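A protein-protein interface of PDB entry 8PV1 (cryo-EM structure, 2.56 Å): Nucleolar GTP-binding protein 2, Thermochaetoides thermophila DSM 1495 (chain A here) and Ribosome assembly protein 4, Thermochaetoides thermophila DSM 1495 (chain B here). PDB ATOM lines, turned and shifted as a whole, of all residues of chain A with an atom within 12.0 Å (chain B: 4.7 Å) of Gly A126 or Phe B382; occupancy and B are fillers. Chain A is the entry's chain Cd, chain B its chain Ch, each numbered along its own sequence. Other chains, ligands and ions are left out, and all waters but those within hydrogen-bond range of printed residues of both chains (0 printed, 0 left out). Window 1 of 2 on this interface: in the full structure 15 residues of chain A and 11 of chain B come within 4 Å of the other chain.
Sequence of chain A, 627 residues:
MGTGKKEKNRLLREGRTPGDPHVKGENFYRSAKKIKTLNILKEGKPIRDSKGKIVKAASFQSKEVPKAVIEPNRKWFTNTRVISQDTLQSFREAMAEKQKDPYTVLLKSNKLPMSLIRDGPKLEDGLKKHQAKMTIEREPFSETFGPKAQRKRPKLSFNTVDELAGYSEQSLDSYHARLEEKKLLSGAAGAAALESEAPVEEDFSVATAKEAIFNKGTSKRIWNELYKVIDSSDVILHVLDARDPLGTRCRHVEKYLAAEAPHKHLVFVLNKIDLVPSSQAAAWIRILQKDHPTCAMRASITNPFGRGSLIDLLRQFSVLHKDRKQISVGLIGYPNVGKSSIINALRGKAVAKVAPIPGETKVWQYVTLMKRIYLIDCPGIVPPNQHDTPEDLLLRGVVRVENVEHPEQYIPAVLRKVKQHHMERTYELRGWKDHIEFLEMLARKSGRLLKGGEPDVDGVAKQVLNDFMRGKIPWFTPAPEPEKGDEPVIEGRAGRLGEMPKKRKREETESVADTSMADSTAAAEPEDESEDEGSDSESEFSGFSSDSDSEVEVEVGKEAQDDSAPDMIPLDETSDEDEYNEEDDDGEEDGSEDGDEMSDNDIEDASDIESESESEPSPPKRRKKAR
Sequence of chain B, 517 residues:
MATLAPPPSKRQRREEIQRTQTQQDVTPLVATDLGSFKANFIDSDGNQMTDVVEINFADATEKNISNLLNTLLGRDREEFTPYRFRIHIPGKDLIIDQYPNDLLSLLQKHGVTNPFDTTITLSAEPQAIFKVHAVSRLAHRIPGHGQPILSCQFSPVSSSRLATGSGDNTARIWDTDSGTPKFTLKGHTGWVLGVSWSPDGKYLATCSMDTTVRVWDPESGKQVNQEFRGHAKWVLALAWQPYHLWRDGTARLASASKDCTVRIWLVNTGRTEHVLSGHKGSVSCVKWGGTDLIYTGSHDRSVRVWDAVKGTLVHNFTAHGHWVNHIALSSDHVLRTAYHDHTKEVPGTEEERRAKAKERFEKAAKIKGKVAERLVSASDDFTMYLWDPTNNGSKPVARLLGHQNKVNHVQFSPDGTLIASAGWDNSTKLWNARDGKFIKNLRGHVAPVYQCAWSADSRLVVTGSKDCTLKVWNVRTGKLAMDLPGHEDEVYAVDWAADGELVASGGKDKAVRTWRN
O of Pro A121 is in hydrogen-bond range of NE2 of Gln B404 (3.2 Å).
The backbone carbonyl oxygen (O) of Lys A122 lies within hydrogen-bond range of the side-chain amide nitrogen (NE2) of Gln B404, at 3.4 Å.
OD2 of Asp B381 sits close to OG of Ser B379, at 3.4 Å.
The side-chain amide oxygen (OE1) of Gln A131 lies close to the side-chain sulfur (SD) of Met A134 (3.6 Å).
OG1 of Thr B383 sits at hydrogen-bond distance from OD1 of Asp B381 (2.4 Å).
CA of Leu A123 touches OE1 of Gln B404, at 3.3 Å.
Gly A126 touches Phe B382 (O to CE2, 3.6 Å).
CA of Gly A126 touches NE2 of Gln B404, at 3.8 Å.
Leu A127 touches Phe B382.
His A130 touches Phe B382.
Met A134 touches Asp B381.
Printed residues of chain B within 4 Å of Pro A121: Gln B404.
Of the printed residues of chain B, Lys A122 touches Gln B404 (3.4 Å).
Of the printed residues of chain B, Leu A123 touches Gln B404.
Gly A126 touches just these residues of chain B: Phe B382 and Gln B404.
Lys A128 touches none of the printed residues of chain B.
Of the printed residues of chain B, Met A134 touches Asp B381.
Glu A137 touches none of the printed residues of chain B.
No residue of chain A comes within 4 Å of Ser B379.
No residue of chain A comes within 4 Å of Asp B380.
Asp B381 touches one residue of chain A.
No residue of chain A comes within 4 Å of Thr B383.
No residue of chain A comes within 4 Å of Met B384.
No residue of chain A comes within 4 Å of His B403.
Gln B404 touches four residues of chain A.
No residue of chain A comes within 4 Å of Asn B405.
No residue of chain A comes within 4 Å of Lys B406.
Val B407 touches none of the printed residues of chain A.
The nearest printed residue of chain B that does not touch Gly A126 is His B403 (6.1 Å).
The nearest residue of chain A that does not touch Phe B382 is Lys A133 (4.4 Å).
Of the 20 printed residues of chain A, 7 touch a printed residue of chain B.
Printed residues of chain A that touch a printed residue of chain B: Pro A121, Lys A122, Leu A123, Gly A126, Leu A127, His A130 and Met A134.
Among the printed residues, 8 pairs touch across the chains.
Among the printed residues, no Asp or Glu carboxylate lies within 4 Å of a Lys or Arg side-chain nitrogen of the other chain.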
ATOM      1  N   ASP A 119     -26.365  -5.498 -39.565  1.00  0.00           N
ATOM      2  CA  ASP A 119     -26.426  -5.522 -38.114  1.00  0.00           C
ATOM      3  C   ASP A 119     -26.357  -4.107 -37.536  1.00  0.00           C
ATOM      4  O   ASP A 119     -25.834  -3.174 -38.152  1.00  0.00           O
ATOM      5  CB  ASP A 119     -25.330  -6.434 -37.545  1.00  0.00           C
ATOM      6  CG  ASP A 119     -23.910  -5.971 -37.876  1.00  0.00           C
ATOM      7  OD1 ASP A 119     -23.713  -4.965 -38.588  1.00  0.00           O
ATOM      8  OD2 ASP A 119     -22.965  -6.638 -37.405  1.00  0.00           O
ATOM      9  N   GLY A 120     -26.928  -3.952 -36.351  1.00  0.00           N
ATOM     10  CA  GLY A 120     -27.019  -2.656 -35.722  1.00  0.00           C
ATOM     11  C   GLY A 120     -25.678  -2.167 -35.229  1.00  0.00           C
ATOM     12  O   GLY A 120     -24.687  -2.910 -35.150  1.00  0.00           O
ATOM     13  N   PRO A 121     -25.624  -0.881 -34.893  1.00  0.00           N
ATOM     14  CA  PRO A 121     -24.388  -0.314 -34.349  1.00  0.00           C
ATOM     15  C   PRO A 121     -24.117  -0.821 -32.940  1.00  0.00           C
ATOM     16  O   PRO A 121     -24.976  -1.411 -32.281  1.00  0.00           O
ATOM     17  CB  PRO A 121     -24.654   1.195 -34.356  1.00  0.00           C
ATOM     18  CG  PRO A 121     -26.136   1.312 -34.285  1.00  0.00           C
ATOM     19  CD  PRO A 121     -26.681   0.135 -35.045  1.00  0.00           C
ATOM     20  N   LYS A 122     -22.884  -0.594 -32.492  1.00  0.00           N
ATOM     21  CA  LYS A 122     -22.487  -1.001 -31.151  1.00  0.00           C
ATOM     22  C   LYS A 122     -23.229  -0.181 -30.100  1.00  0.00           C
ATOM     23  O   LYS A 122     -23.630   0.962 -30.338  1.00  0.00           O
ATOM     24  CB  LYS A 122     -20.977  -0.849 -30.978  1.00  0.00           C
ATOM     25  CG  LYS A 122     -20.163  -1.571 -32.040  1.00  0.00           C
ATOM     26  CD  LYS A 122     -18.675  -1.300 -31.887  1.00  0.00           C
ATOM     27  CE  LYS A 122     -17.872  -2.009 -32.966  1.00  0.00           C
ATOM     28  NZ  LYS A 122     -16.416  -1.720 -32.848  1.00  0.00           N
ATOM     29  N   LEU A 123     -23.417  -0.791 -28.923  1.00  0.00           N
ATOM     30  CA  LEU A 123     -24.219  -0.166 -27.875  1.00  0.00           C
ATOM     31  C   LEU A 123     -23.532   1.072 -27.309  1.00  0.00           C
ATOM     32  O   LEU A 123     -24.200   2.045 -26.941  1.00  0.00           O
ATOM     33  CB  LEU A 123     -24.537  -1.191 -26.778  1.00  0.00           C
ATOM     34  CG  LEU A 123     -23.458  -1.904 -25.948  1.00  0.00           C
ATOM     35  CD1 LEU A 123     -22.982  -1.103 -24.731  1.00  0.00           C
ATOM     36  CD2 LEU A 123     -23.943  -3.285 -25.531  1.00  0.00           C
ATOM     37  N   GLU A 124     -22.198   1.055 -27.244  1.00  0.00           N
ATOM     38  CA  GLU A 124     -21.456   2.235 -26.810  1.00  0.00           C
ATOM     39  C   GLU A 124     -21.663   3.396 -27.781  1.00  0.00           C
ATOM     40  O   GLU A 124     -21.883   4.543 -27.367  1.00  0.00           O
ATOM     41  CB  GLU A 124     -19.969   1.895 -26.661  1.00  0.00           C
ATOM     42  CG  GLU A 124     -19.354   1.082 -27.812  1.00  0.00           C
ATOM     43  CD  GLU A 124     -19.400  -0.417 -27.576  1.00  0.00           C
ATOM     44  OE1 GLU A 124     -20.101  -0.848 -26.638  1.00  0.00           O
ATOM     45  OE2 GLU A 124     -18.729  -1.165 -28.319  1.00  0.00           O
ATOM     46  N   ASP A 125     -21.629   3.104 -29.083  1.00  0.00           N
ATOM     47  CA  ASP A 125     -21.883   4.137 -30.081  1.00  0.00           C
ATOM     48  C   ASP A 125     -23.315   4.650 -29.990  1.00  0.00           C
ATOM     49  O   ASP A 125     -23.549   5.862 -30.054  1.00  0.00           O
ATOM     50  CB  ASP A 125     -21.585   3.600 -31.480  1.00  0.00           C
ATOM     51  CG  ASP A 125     -20.099   3.382 -31.717  1.00  0.00           C
ATOM     52  OD1 ASP A 125     -19.280   4.112 -31.121  1.00  0.00           O
ATOM     53  OD2 ASP A 125     -19.745   2.477 -32.500  1.00  0.00           O
ATOM     54  N   GLY A 126     -24.277   3.748 -29.783  1.00  0.00           N
ATOM     55  CA  GLY A 126     -25.667   4.167 -29.684  1.00  0.00           C
ATOM     56  C   GLY A 126     -25.978   4.920 -28.403  1.00  0.00           C
ATOM     57  O   GLY A 126     -26.978   5.635 -28.320  1.00  0.00           O
ATOM     58  N   LEU A 127     -25.142   4.749 -27.377  1.00  0.00           N
ATOM     59  CA  LEU A 127     -25.372   5.477 -26.134  1.00  0.00           C
ATOM     60  C   LEU A 127     -24.736   6.863 -26.167  1.00  0.00           C
ATOM     61  O   LEU A 127     -25.400   7.856 -25.838  1.00  0.00           O
ATOM     62  CB  LEU A 127     -24.849   4.670 -24.948  1.00  0.00           C
ATOM     63  CG  LEU A 127     -25.889   3.758 -24.293  1.00  0.00           C
ATOM     64  CD1 LEU A 127     -25.258   2.938 -23.185  1.00  0.00           C
ATOM     65  CD2 LEU A 127     -27.065   4.564 -23.771  1.00  0.00           C
ATOM     66  N   LYS A 128     -23.463   6.959 -26.570  1.00  0.00           N
ATOM     67  CA  LYS A 128     -22.845   8.281 -26.681  1.00  0.00           C
ATOM     68  C   LYS A 128     -23.339   9.052 -27.900  1.00  0.00           C
ATOM     69  O   LYS A 128     -23.044  10.243 -28.040  1.00  0.00           O
ATOM     70  CB  LYS A 128     -21.315   8.200 -26.667  1.00  0.00           C
ATOM     71  CG  LYS A 128     -20.710   8.135 -25.260  1.00  0.00           C
ATOM     72  CD  LYS A 128     -20.868   6.816 -24.537  1.00  0.00           C
ATOM     73  CE  LYS A 128     -20.024   5.741 -25.166  1.00  0.00           C
ATOM     74  NZ  LYS A 128     -20.126   4.455 -24.425  1.00  0.00           N
ATOM     75  N   LYS A 129     -24.092   8.406 -28.794  1.00  0.00           N
ATOM     76  CA  LYS A 129     -24.780   9.160 -29.830  1.00  0.00           C
ATOM     77  C   LYS A 129     -25.909  10.009 -29.258  1.00  0.00           C
ATOM     78  O   LYS A 129     -26.227  11.065 -29.818  1.00  0.00           O
ATOM     79  CB  LYS A 129     -25.312   8.192 -30.891  1.00  0.00           C
ATOM     80  CG  LYS A 129     -25.938   8.848 -32.103  1.00  0.00           C
ATOM     81  CD  LYS A 129     -26.382   7.812 -33.115  1.00  0.00           C
ATOM     82  CE  LYS A 129     -26.931   8.478 -34.361  1.00  0.00           C
ATOM     83  NZ  LYS A 129     -28.204   9.196 -34.070  1.00  0.00           N
ATOM     84  N   HIS A 130     -26.496   9.592 -28.137  1.00  0.00           N
ATOM     85  CA  HIS A 130     -27.675  10.242 -27.587  1.00  0.00           C
ATOM     86  C   HIS A 130     -27.473  10.821 -26.193  1.00  0.00           C
ATOM     87  O   HIS A 130     -28.432  11.370 -25.633  1.00  0.00           O
ATOM     88  CB  HIS A 130     -28.847   9.254 -27.553  1.00  0.00           C
ATOM     89  CG  HIS A 130     -29.270   8.767 -28.904  1.00  0.00           C
ATOM     90  ND1 HIS A 130     -30.207   9.423 -29.673  1.00  0.00           N
ATOM     91  CD2 HIS A 130     -28.891   7.683 -29.622  1.00  0.00           C
ATOM     92  CE1 HIS A 130     -30.385   8.766 -30.805  1.00  0.00           C
ATOM     93  NE2 HIS A 130     -29.597   7.707 -30.799  1.00  0.00           N
ATOM     94  N   GLN A 131     -26.272  10.692 -25.612  1.00  0.00           N
ATOM     95  CA  GLN A 131     -26.013  11.231 -24.274  1.00  0.00           C
ATOM     96  C   GLN A 131     -26.258  12.734 -24.190  1.00  0.00           C
ATOM     97  O   GLN A 131     -26.794  13.222 -23.188  1.00  0.00           O
ATOM     98  CB  GLN A 131     -24.579  10.922 -23.841  1.00  0.00           C
ATOM     99  CG  GLN A 131     -24.356   9.519 -23.321  1.00  0.00           C
ATOM    100  CD  GLN A 131     -25.242   9.187 -22.139  1.00  0.00           C
ATOM    101  OE1 GLN A 131     -26.174   8.392 -22.252  1.00  0.00           O
ATOM    102  NE2 GLN A 131     -24.956   9.798 -20.996  1.00  0.00           N
ATOM    103  N   ALA A 132     -25.867  13.485 -25.223  1.00  0.00           N
ATOM    104  CA  ALA A 132     -25.996  14.940 -25.179  1.00  0.00           C
ATOM    105  C   ALA A 132     -27.458  15.371 -25.130  1.00  0.00           C
ATOM    106  O   ALA A 132     -27.859  16.155 -24.256  1.00  0.00           O
ATOM    107  CB  ALA A 132     -25.290  15.565 -26.382  1.00  0.00           C
ATOM    108  N   LYS A 133     -28.280  14.846 -26.046  1.00  0.00           N
ATOM    109  CA  LYS A 133     -29.689  15.223 -26.055  1.00  0.00           C
ATOM    110  C   LYS A 133     -30.403  14.658 -24.836  1.00  0.00           C
ATOM    111  O   LYS A 133     -31.380  15.242 -24.358  1.00  0.00           O
ATOM    112  CB  LYS A 133     -30.362  14.775 -27.362  1.00  0.00           C
ATOM    113  CG  LYS A 133     -30.467  13.266 -27.646  1.00  0.00           C
ATOM    114  CD  LYS A 133     -31.772  12.653 -27.104  1.00  0.00           C
ATOM    115  CE  LYS A 133     -31.925  11.193 -27.473  1.00  0.00           C
ATOM    116  NZ  LYS A 133     -33.175  10.596 -26.931  1.00  0.00           N
ATOM    117  N   MET A 134     -29.921  13.527 -24.314  1.00  0.00           N
ATOM    118  CA  MET A 134     -30.494  12.959 -23.101  1.00  0.00           C
ATOM    119  C   MET A 134     -30.273  13.877 -21.906  1.00  0.00           C
ATOM    120  O   MET A 134     -31.196  14.109 -21.115  1.00  0.00           O
ATOM    121  CB  MET A 134     -29.876  11.587 -22.857  1.00  0.00           C
ATOM    122  CG  MET A 134     -30.450  10.799 -21.709  1.00  0.00           C
ATOM    123  SD  MET A 134     -29.569   9.233 -21.632  1.00  0.00           S
ATOM    124  CE  MET A 134     -30.228   8.428 -23.091  1.00  0.00           C
ATOM    125  N   THR A 135     -29.060  14.425 -21.772  1.00  0.00           N
ATOM    126  CA  THR A 135     -28.783  15.374 -20.696  1.00  0.00           C
ATOM    127  C   THR A 135     -29.582  16.662 -20.864  1.00  0.00           C
ATOM    128  O   THR A 135     -30.081  17.223 -19.879  1.00  0.00           O
ATOM    129  CB  THR A 135     -27.288  15.684 -20.632  1.00  0.00           C
ATOM    130  OG1 THR A 135     -26.823  16.079 -21.927  1.00  0.00           O
ATOM    131  CG2 THR A 135     -26.507  14.470 -20.161  1.00  0.00           C
ATOM    132  N   ILE A 136     -29.714  17.146 -22.103  1.00  0.00           N
ATOM    133  CA  ILE A 136     -30.478  18.374 -22.325  1.00  0.00           C
ATOM    134  C   ILE A 136     -31.965  18.157 -22.038  1.00  0.00           C
ATOM    135  O   ILE A 136     -32.632  19.041 -21.485  1.00  0.00           O
ATOM    136  CB  ILE A 136     -30.231  18.905 -23.751  1.00  0.00           C
ATOM    137  CG1 ILE A 136     -28.750  19.227 -23.944  1.00  0.00           C
ATOM    138  CG2 ILE A 136     -31.045  20.159 -24.025  1.00  0.00           C
ATOM    139  CD1 ILE A 136     -28.173  20.137 -22.881  1.00  0.00           C
ATOM    140  N   GLU A 137     -32.502  16.983 -22.382  1.00  0.00           N
ATOM    141  CA  GLU A 137     -33.887  16.665 -22.045  1.00  0.00           C
ATOM    142  C   GLU A 137     -34.077  16.518 -20.542  1.00  0.00           C
ATOM    143  O   GLU A 137     -35.110  16.929 -20.001  1.00  0.00           O
ATOM    144  CB  GLU A 137     -34.322  15.385 -22.756  1.00  0.00           C
ATOM    145  CG  GLU A 137     -34.665  15.562 -24.221  1.00  0.00           C
ATOM    146  CD  GLU A 137     -34.854  14.239 -24.935  1.00  0.00           C
ATOM    147  OE1 GLU A 137     -34.459  13.195 -24.372  1.00  0.00           O
ATOM    148  OE2 GLU A 137     -35.397  14.240 -26.060  1.00  0.00           O
ATOM    149  N   ARG A 138     -33.103  15.914 -19.854  1.00  0.00           N
ATOM    150  CA  ARG A 138     -33.209  15.741 -18.409  1.00  0.00           C
ATOM    151  C   ARG A 138     -33.183  17.077 -17.681  1.00  0.00           C
ATOM    152  O   ARG A 138     -33.970  17.301 -16.756  1.00  0.00           O
ATOM    153  CB  ARG A 138     -32.086  14.840 -17.905  1.00  0.00           C
ATOM    154  CG  ARG A 138     -32.144  14.564 -16.416  1.00  0.00           C
ATOM    155  CD  ARG A 138     -30.823  14.042 -15.873  1.00  0.00           C
ATOM    156  NE  ARG A 138     -30.188  13.079 -16.764  1.00  0.00           N
ATOM    157  CZ  ARG A 138     -29.042  13.283 -17.398  1.00  0.00           C
ATOM    158  NH1 ARG A 138     -28.367  14.411 -17.258  1.00  0.00           N
ATOM    159  NH2 ARG A 138     -28.562  12.333 -18.194  1.00  0.00           N
ATOM    160  N   SER B 379     -36.304   2.130 -18.706  1.00  0.00           N
ATOM    161  CA  SER B 379     -36.370   3.580 -18.793  1.00  0.00           C
ATOM    162  C   SER B 379     -36.053   4.075 -20.194  1.00  0.00           C
ATOM    163  O   SER B 379     -35.571   3.334 -21.054  1.00  0.00           O
ATOM    164  CB  SER B 379     -35.423   4.243 -17.793  1.00  0.00           C
ATOM    165  OG  SER B 379     -34.156   3.619 -17.825  1.00  0.00           O
ATOM    166  N   ASP B 380     -36.339   5.359 -20.402  1.00  0.00           N
ATOM    167  CA  ASP B 380     -36.062   6.151 -21.592  1.00  0.00           C
ATOM    168  C   ASP B 380     -34.601   6.480 -21.752  1.00  0.00           C
ATOM    169  O   ASP B 380     -34.234   7.019 -22.801  1.00  0.00           O
ATOM    170  CB  ASP B 380     -36.878   7.443 -21.566  1.00  0.00           C
ATOM    171  CG  ASP B 380     -38.264   7.270 -22.139  1.00  0.00           C
ATOM    172  OD1 ASP B 380     -38.602   6.143 -22.553  1.00  0.00           O
ATOM    173  OD2 ASP B 380     -39.015   8.264 -22.183  1.00  0.00           O
ATOM    174  N   ASP B 381     -33.743   6.188 -20.775  1.00  0.00           N
ATOM    175  CA  ASP B 381     -32.305   6.355 -20.935  1.00  0.00           C
ATOM    176  C   ASP B 381     -31.651   5.165 -21.630  1.00  0.00           C
ATOM    177  O   ASP B 381     -30.448   4.947 -21.452  1.00  0.00           O
ATOM    178  CB  ASP B 381     -31.636   6.632 -19.579  1.00  0.00           C
ATOM    179  CG  ASP B 381     -31.836   5.518 -18.556  1.00  0.00           C
ATOM    180  OD1 ASP B 381     -32.323   4.419 -18.887  1.00  0.00           O
ATOM    181  OD2 ASP B 381     -31.485   5.748 -17.382  1.00  0.00           O
ATOM    182  N   PHE B 382     -32.448   4.381 -22.364  1.00  0.00           N
ATOM    183  CA  PHE B 382     -32.089   3.256 -23.226  1.00  0.00           C
ATOM    184  C   PHE B 382     -31.765   2.010 -22.415  1.00  0.00           C
ATOM    185  O   PHE B 382     -31.337   1.000 -22.982  1.00  0.00           O
ATOM    186  CB  PHE B 382     -30.902   3.536 -24.163  1.00  0.00           C
ATOM    187  CG  PHE B 382     -31.150   4.612 -25.187  1.00  0.00           C
ATOM    188  CD1 PHE B 382     -32.413   5.124 -25.416  1.00  0.00           C
ATOM    189  CD2 PHE B 382     -30.107   5.062 -25.975  1.00  0.00           C
ATOM    190  CE1 PHE B 382     -32.619   6.105 -26.361  1.00  0.00           C
ATOM    191  CE2 PHE B 382     -30.312   6.029 -26.931  1.00  0.00           C
ATOM    192  CZ  PHE B 382     -31.570   6.550 -27.126  1.00  0.00           C
ATOM    193  N   THR B 383     -31.948   2.048 -21.096  1.00  0.00           N
ATOM    194  CA  THR B 383     -31.390   1.034 -20.213  1.00  0.00           C
ATOM    195  C   THR B 383     -32.469   0.442 -19.319  1.00  0.00           C
ATOM    196  O   THR B 383     -33.634   0.868 -19.317  1.00  0.00           O
ATOM    197  CB  THR B 383     -30.272   1.600 -19.323  1.00  0.00           C
ATOM    198  OG1 THR B 383     -30.819   2.583 -18.437  1.00  0.00           O
ATOM    199  CG2 THR B 383     -29.181   2.243 -20.154  1.00  0.00           C
ATOM    200  N   MET B 384     -32.052  -0.569 -18.558  1.00  0.00           N
ATOM    201  CA  MET B 384     -32.875  -1.160 -17.516  1.00  0.00           C
ATOM    202  C   MET B 384     -32.027  -1.371 -16.273  1.00  0.00           C
ATOM    203  O   MET B 384     -30.801  -1.438 -16.347  1.00  0.00           O
ATOM    204  CB  MET B 384     -33.483  -2.487 -17.973  1.00  0.00           C
ATOM    205  CG  MET B 384     -34.512  -2.337 -19.067  1.00  0.00           C
ATOM    206  SD  MET B 384     -35.144  -3.920 -19.597  1.00  0.00           S
ATOM    207  CE  MET B 384     -33.720  -4.464 -20.521  1.00  0.00           C
ATOM    208  N   HIS B 403     -30.121  -1.988 -25.643  1.00  0.00           N
ATOM    209  CA  HIS B 403     -31.128  -1.343 -26.473  1.00  0.00           C
ATOM    210  C   HIS B 403     -30.593  -0.033 -27.037  1.00  0.00           C
ATOM    211  O   HIS B 403     -29.953   0.751 -26.332  1.00  0.00           O
ATOM    212  CB  HIS B 403     -32.399  -1.088 -25.668  1.00  0.00           C
ATOM    213  CG  HIS B 403     -33.309  -2.274 -25.579  1.00  0.00           C
ATOM    214  ND1 HIS B 403     -34.163  -2.634 -26.600  1.00  0.00           N
ATOM    215  CD2 HIS B 403     -33.497  -3.182 -24.594  1.00  0.00           C
ATOM    216  CE1 HIS B 403     -34.840  -3.711 -26.245  1.00  0.00           C
ATOM    217  NE2 HIS B 403     -34.455  -4.063 -25.032  1.00  0.00           N
ATOM    218  N   GLN B 404     -30.856   0.200 -28.322  1.00  0.00           N
ATOM    219  CA  GLN B 404     -30.412   1.406 -29.006  1.00  0.00           C
ATOM    220  C   GLN B 404     -31.471   2.498 -28.988  1.00  0.00           C
ATOM    221  O   GLN B 404     -31.255   3.580 -29.541  1.00  0.00           O
ATOM    222  CB  GLN B 404     -30.009   1.083 -30.444  1.00  0.00           C
ATOM    223  CG  GLN B 404     -29.119  -0.134 -30.571  1.00  0.00           C
ATOM    224  CD  GLN B 404     -27.702   0.143 -30.130  1.00  0.00           C
ATOM    225  OE1 GLN B 404     -27.304  -0.227 -29.029  1.00  0.00           O
ATOM    226  NE2 GLN B 404     -26.932   0.803 -30.984  1.00  0.00           N
ATOM    227  N   ASN B 405     -32.614   2.236 -28.368  1.00  0.00           N
ATOM    228  CA  ASN B 405     -33.653   3.241 -28.209  1.00  0.00           C
ATOM    229  C   ASN B 405     -34.372   2.955 -26.898  1.00  0.00           C
ATOM    230  O   ASN B 405     -33.973   2.070 -26.136  1.00  0.00           O
ATOM    231  CB  ASN B 405     -34.603   3.259 -29.406  1.00  0.00           C
ATOM    232  CG  ASN B 405     -35.181   4.633 -29.663  1.00  0.00           C
ATOM    233  OD1 ASN B 405     -35.285   5.453 -28.753  1.00  0.00           O
ATOM    234  ND2 ASN B 405     -35.555   4.895 -30.908  1.00  0.00           N
ATOM    235  N   LYS B 406     -35.412   3.740 -26.624  1.00  0.00           N
ATOM    236  CA  LYS B 406     -36.117   3.666 -25.350  1.00  0.00           C
ATOM    237  C   LYS B 406     -36.775   2.306 -25.171  1.00  0.00           C
ATOM    238  O   LYS B 406     -37.273   1.708 -26.127  1.00  0.00           O
ATOM    239  CB  LYS B 406     -37.168   4.770 -25.270  1.00  0.00           C
ATOM    240  CG  LYS B 406     -36.645   6.143 -25.634  1.00  0.00           C
ATOM    241  CD  LYS B 406     -37.750   7.184 -25.619  1.00  0.00           C
ATOM    242  CE  LYS B 406     -38.735   6.967 -26.748  1.00  0.00           C
ATOM    243  NZ  LYS B 406     -38.096   7.170 -28.075  1.00  0.00           N
ATOM    244  N   VAL B 407     -36.759   1.807 -23.940  1.00  0.00           N
ATOM    245  CA  VAL B 407     -37.330   0.506 -23.622  1.00  0.00           C
ATOM    246  C   VAL B 407     -38.729   0.746 -23.076  1.00  0.00           C
ATOM    247  O   VAL B 407     -38.900   1.428 -22.060  1.00  0.00           O
ATOM    248  CB  VAL B 407     -36.466  -0.262 -22.612  1.00  0.00           C
ATOM    249  CG1 VAL B 407     -37.085  -1.617 -22.316  1.00  0.00           C
ATOM    250  CG2 VAL B 407     -35.048  -0.399 -23.114  1.00  0.00           C
